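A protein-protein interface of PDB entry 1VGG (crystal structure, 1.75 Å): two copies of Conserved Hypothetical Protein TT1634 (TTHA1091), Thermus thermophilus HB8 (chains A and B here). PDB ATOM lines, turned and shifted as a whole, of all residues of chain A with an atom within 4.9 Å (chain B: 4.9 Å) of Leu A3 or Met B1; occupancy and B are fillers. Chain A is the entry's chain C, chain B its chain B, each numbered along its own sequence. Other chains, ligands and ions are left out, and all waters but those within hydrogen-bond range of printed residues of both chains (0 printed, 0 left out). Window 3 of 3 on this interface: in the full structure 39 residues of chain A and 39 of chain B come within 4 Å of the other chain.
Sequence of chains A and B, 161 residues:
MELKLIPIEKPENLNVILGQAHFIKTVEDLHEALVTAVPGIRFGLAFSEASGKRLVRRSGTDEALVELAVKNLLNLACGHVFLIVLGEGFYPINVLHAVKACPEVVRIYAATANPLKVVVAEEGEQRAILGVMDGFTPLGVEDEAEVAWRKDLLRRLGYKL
Leu A3 touches Met B1, but with the chains exchanged Met A1 does not touch Leu B3 (8.0 Å).
Positions printed for both chains: 1, 2, 3 and 121.
Among the printed residues, pairs that only touch across the chains: Leu A5 with Glu B123 (3.6 Å), Met A133 with Glu B123 (3.6 Å), Met A133 with Ala B121 (3.8 Å), Val A119 with Met B1 (3.9 Å), Leu A3 with Met B1 (3.9 Å), Met A133 with Glu B122 (3.96 Å) and Met A133 with Met B1 (3.98 Å).
Of chain B, only Met B1 (3.9 Å) comes within 4 Å of Leu A3.
Printed residues of chain B within 4 Å of Val A119: Met B1 (3.9 Å).
Of the printed residues of chain B, Met A133 touches Met B1 (3.98 Å), Ala B121 (3.8 Å), Glu B122 (3.96 Å) and Glu B123 (3.6 Å).
Of the printed residues of chain A, Glu B123 touches Leu A5 and Met A133.
Of the printed residues of chain A, Ala B121 touches Met A133.
Ala A121 touches none of the printed residues of chain B.
The nearest residue of chain B that does not touch Leu A3 is Leu B3 (4.3 Å).
N of Met B1 is in hydrogen-bond range of OE1 of Glu B123 (2.6 Å).
O of Glu B2 lies within hydrogen-bond range of N of Glu B122 (2.8 Å).
The backbone carbonyl oxygen (O) of Val A119 sits at hydrogen-bond distance from the backbone NH (N) of Leu A130 (2.8 Å).
Of the 6 printed residues of chain B, 4 touch a printed residue of chain A.
Hydrophobic or aromatic side chains of chain B within 4 Å of the printed part of chain A: Met B1 and Ala B121.
Of the 10 printed residues of chain A, 4 touch a printed residue of chain B.
Hydrophobic or aromatic side chains of chain A within 4 Å of the printed part of chain B: Leu A3, Leu A5, Val A119 and Met A133.
Among the printed residues, no Asp or Glu carboxylate lies within 4 Å of a Lys or Arg side-chain nitrogen of the other chain.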
ATOM      1  N   MET A   1      31.870 -19.527 -33.884  1.00  0.00           N
ATOM      2  CA  MET A   1      31.408 -20.740 -33.136  1.00  0.00           C
ATOM      3  C   MET A   1      29.937 -20.614 -32.746  1.00  0.00           C
ATOM      4  O   MET A   1      29.463 -19.533 -32.392  1.00  0.00           O
ATOM      5  CB  MET A   1      32.264 -20.935 -31.882  1.00  0.00           C
ATOM      6  CG  MET A   1      31.887 -22.139 -31.039  1.00  0.00           C
ATOM      7  SD  MET A   1      33.058 -22.363 -29.497  1.00  0.00           S
ATOM      8  CE  MET A   1      32.014 -21.405 -28.190  1.00  0.00           C
ATOM      9  N   GLU A   2      29.211 -21.721 -32.817  1.00  0.00           N
ATOM     10  CA  GLU A   2      27.804 -21.703 -32.461  1.00  0.00           C
ATOM     11  C   GLU A   2      27.446 -22.929 -31.641  1.00  0.00           C
ATOM     12  O   GLU A   2      28.066 -23.986 -31.785  1.00  0.00           O
ATOM     13  CB  GLU A   2      26.927 -21.642 -33.715  1.00  0.00           C
ATOM     14  CG  GLU A   2      27.046 -22.836 -34.639  1.00  0.00           C
ATOM     15  CD  GLU A   2      25.950 -22.852 -35.692  1.00  0.00           C
ATOM     16  OE1 GLU A   2      25.772 -21.828 -36.386  1.00  0.00           O
ATOM     17  OE2 GLU A   2      25.265 -23.891 -35.825  1.00  0.00           O
ATOM     18  N   LEU A   3      26.447 -22.774 -30.779  1.00  0.00           N
ATOM     19  CA  LEU A   3      25.993 -23.868 -29.928  1.00  0.00           C
ATOM     20  C   LEU A   3      24.705 -24.455 -30.492  1.00  0.00           C
ATOM     21  O   LEU A   3      23.851 -23.725 -31.002  1.00  0.00           O
ATOM     22  CB  LEU A   3      25.745 -23.370 -28.503  1.00  0.00           C
ATOM     23  CG  LEU A   3      26.921 -22.719 -27.767  1.00  0.00           C
ATOM     24  CD1 LEU A   3      26.529 -22.461 -26.319  1.00  0.00           C
ATOM     25  CD2 LEU A   3      28.134 -23.632 -27.818  1.00  0.00           C
ATOM     26  N   LYS A   4      24.576 -25.774 -30.413  1.00  0.00           N
ATOM     27  CA  LYS A   4      23.388 -26.455 -30.916  1.00  0.00           C
ATOM     28  C   LYS A   4      22.946 -27.500 -29.903  1.00  0.00           C
ATOM     29  O   LYS A   4      23.733 -27.920 -29.057  1.00  0.00           O
ATOM     30  CB  LYS A   4      23.691 -27.121 -32.258  1.00  0.00           C
ATOM     31  CG  LYS A   4      23.909 -26.116 -33.397  1.00  0.00           C
ATOM     32  CD  LYS A   4      24.558 -26.757 -34.602  1.00  0.00           C
ATOM     33  CE  LYS A   4      25.932 -27.294 -34.241  1.00  0.00           C
ATOM     34  NZ  LYS A   4      26.687 -27.726 -35.446  1.00  0.00           N
ATOM     35  N   LEU A   5      21.685 -27.903 -29.988  1.00  0.00           N
ATOM     36  CA  LEU A   5      21.143 -28.908 -29.087  1.00  0.00           C
ATOM     37  C   LEU A   5      20.649 -30.058 -29.963  1.00  0.00           C
ATOM     38  O   LEU A   5      19.687 -29.904 -30.731  1.00  0.00           O
ATOM     39  CB  LEU A   5      19.997 -28.308 -28.269  1.00  0.00           C
ATOM     40  CG  LEU A   5      19.448 -29.132 -27.103  1.00  0.00           C
ATOM     41  CD1 LEU A   5      20.572 -29.470 -26.116  1.00  0.00           C
ATOM     42  CD2 LEU A   5      18.354 -28.333 -26.402  1.00  0.00           C
ATOM     43  N   VAL A 119      24.391 -31.073 -25.909  1.00  0.00           N
ATOM     44  CA  VAL A 119      24.764 -29.693 -26.190  1.00  0.00           C
ATOM     45  C   VAL A 119      26.088 -29.774 -26.931  1.00  0.00           C
ATOM     46  O   VAL A 119      27.036 -30.382 -26.436  1.00  0.00           O
ATOM     47  CB  VAL A 119      24.983 -28.896 -24.896  1.00  0.00           C
ATOM     48  CG1 VAL A 119      25.379 -27.455 -25.227  1.00  0.00           C
ATOM     49  CG2 VAL A 119      23.725 -28.928 -24.049  1.00  0.00           C
ATOM     50  N   VAL A 120      26.161 -29.170 -28.112  1.00  0.00           N
ATOM     51  CA  VAL A 120      27.399 -29.209 -28.885  1.00  0.00           C
ATOM     52  C   VAL A 120      27.833 -27.819 -29.326  1.00  0.00           C
ATOM     53  O   VAL A 120      27.009 -26.916 -29.455  1.00  0.00           O
ATOM     54  CB  VAL A 120      27.237 -30.063 -30.166  1.00  0.00           C
ATOM     55  CG1 VAL A 120      26.782 -31.469 -29.807  1.00  0.00           C
ATOM     56  CG2 VAL A 120      26.245 -29.396 -31.115  1.00  0.00           C
ATOM     57  N   ALA A 121      29.135 -27.661 -29.542  1.00  0.00           N
ATOM     58  CA  ALA A 121      29.700 -26.409 -30.026  1.00  0.00           C
ATOM     59  C   ALA A 121      30.266 -26.739 -31.402  1.00  0.00           C
ATOM     60  O   ALA A 121      30.883 -27.793 -31.596  1.00  0.00           O
ATOM     61  CB  ALA A 121      30.812 -25.922 -29.100  1.00  0.00           C
ATOM     62  N   LEU A 130      29.599 -30.606 -25.349  1.00  0.00           N
ATOM     63  CA  LEU A 130      29.778 -29.796 -24.146  1.00  0.00           C
ATOM     64  C   LEU A 130      29.080 -30.397 -22.933  1.00  0.00           C
ATOM     65  O   LEU A 130      29.487 -30.174 -21.800  1.00  0.00           O
ATOM     66  CB  LEU A 130      29.263 -28.365 -24.367  1.00  0.00           C
ATOM     67  CG  LEU A 130      29.832 -27.555 -25.539  1.00  0.00           C
ATOM     68  CD1 LEU A 130      29.408 -26.083 -25.386  1.00  0.00           C
ATOM     69  CD2 LEU A 130      31.357 -27.660 -25.568  1.00  0.00           C
ATOM     70  N   MET A 133      21.910 -33.377 -21.647  1.00  0.00           N
ATOM     71  CA  MET A 133      20.696 -33.113 -20.883  1.00  0.00           C
ATOM     72  C   MET A 133      20.103 -34.511 -20.746  1.00  0.00           C
ATOM     73  O   MET A 133      19.473 -35.025 -21.671  1.00  0.00           O
ATOM     74  CB  MET A 133      19.762 -32.194 -21.668  1.00  0.00           C
ATOM     75  CG  MET A 133      20.287 -30.777 -21.759  1.00  0.00           C
ATOM     76  SD  MET A 133      18.992 -29.577 -22.541  1.00  0.00           S
ATOM     77  CE  MET A 133      20.061 -27.950 -22.531  1.00  0.00           C
ATOM     78  N   MET B   1      17.536 -22.109 -25.336  1.00  0.00           N
ATOM     79  CA  MET B   1      18.562 -22.594 -24.370  1.00  0.00           C
ATOM     80  C   MET B   1      19.304 -21.415 -23.736  1.00  0.00           C
ATOM     81  O   MET B   1      19.574 -20.411 -24.395  1.00  0.00           O
ATOM     82  CB  MET B   1      19.548 -23.512 -25.098  1.00  0.00           C
ATOM     83  CG  MET B   1      20.534 -24.220 -24.200  1.00  0.00           C
ATOM     84  SD  MET B   1      21.640 -25.457 -25.204  1.00  0.00           S
ATOM     85  CE  MET B   1      23.159 -24.309 -25.472  1.00  0.00           C
ATOM     86  N   GLU B   2      19.619 -21.534 -22.452  1.00  0.00           N
ATOM     87  CA  GLU B   2      20.334 -20.478 -21.741  1.00  0.00           C
ATOM     88  C   GLU B   2      21.440 -21.080 -20.892  1.00  0.00           C
ATOM     89  O   GLU B   2      21.323 -22.216 -20.442  1.00  0.00           O
ATOM     90  CB  GLU B   2      19.383 -19.696 -20.832  1.00  0.00           C
ATOM     91  CG  GLU B   2      18.288 -18.948 -21.572  1.00  0.00           C
ATOM     92  CD  GLU B   2      17.463 -18.065 -20.655  1.00  0.00           C
ATOM     93  OE1 GLU B   2      16.569 -17.352 -21.164  1.00  0.00           O
ATOM     94  OE2 GLU B   2      17.707 -18.083 -19.426  1.00  0.00           O
ATOM     95  N   LEU B   3      22.515 -20.326 -20.683  1.00  0.00           N
ATOM     96  CA  LEU B   3      23.615 -20.803 -19.854  1.00  0.00           C
ATOM     97  C   LEU B   3      23.547 -20.112 -18.504  1.00  0.00           C
ATOM     98  O   LEU B   3      23.260 -18.916 -18.423  1.00  0.00           O
ATOM     99  CB  LEU B   3      24.969 -20.517 -20.512  1.00  0.00           C
ATOM    100  CG  LEU B   3      25.213 -21.148 -21.885  1.00  0.00           C
ATOM    101  CD1 LEU B   3      26.689 -21.008 -22.245  1.00  0.00           C
ATOM    102  CD2 LEU B   3      24.821 -22.615 -21.866  1.00  0.00           C
ATOM    103  N   ALA B 121      23.608 -25.660 -18.912  1.00  0.00           N
ATOM    104  CA  ALA B 121      22.800 -25.223 -20.046  1.00  0.00           C
ATOM    105  C   ALA B 121      21.387 -25.654 -19.660  1.00  0.00           C
ATOM    106  O   ALA B 121      21.198 -26.733 -19.105  1.00  0.00           O
ATOM    107  CB  ALA B 121      23.234 -25.926 -21.336  1.00  0.00           C
ATOM    108  N   GLU B 122      20.405 -24.797 -19.925  1.00  0.00           N
ATOM    109  CA  GLU B 122      19.022 -25.113 -19.589  1.00  0.00           C
ATOM    110  C   GLU B 122      18.105 -24.970 -20.796  1.00  0.00           C
ATOM    111  O   GLU B 122      18.232 -24.027 -21.573  1.00  0.00           O
ATOM    112  CB  GLU B 122      18.523 -24.196 -18.462  1.00  0.00           C
ATOM    113  CG  GLU B 122      17.060 -24.420 -18.077  1.00  0.00           C
ATOM    114  CD  GLU B 122      16.629 -23.588 -16.880  1.00  0.00           C
ATOM    115  OE1 GLU B 122      15.543 -22.983 -16.941  1.00  0.00           O
ATOM    116  OE2 GLU B 122      17.364 -23.543 -15.873  1.00  0.00           O
ATOM    117  N   GLU B 123      17.195 -25.928 -20.952  1.00  0.00           N
ATOM    118  CA  GLU B 123      16.217 -25.906 -22.036  1.00  0.00           C
ATOM    119  C   GLU B 123      14.983 -26.657 -21.549  1.00  0.00           C
ATOM    120  O   GLU B 123      15.031 -27.869 -21.333  1.00  0.00           O
ATOM    121  CB  GLU B 123      16.778 -26.568 -23.293  1.00  0.00           C
ATOM    122  CG  GLU B 123      15.810 -26.605 -24.479  1.00  0.00           C
ATOM    123  CD  GLU B 123      15.388 -25.225 -24.948  1.00  0.00           C
ATOM    124  OE1 GLU B 123      16.261 -24.342 -25.073  1.00  0.00           O
ATOM    125  OE2 GLU B 123      14.183 -25.022 -25.213  1.00  0.00           O
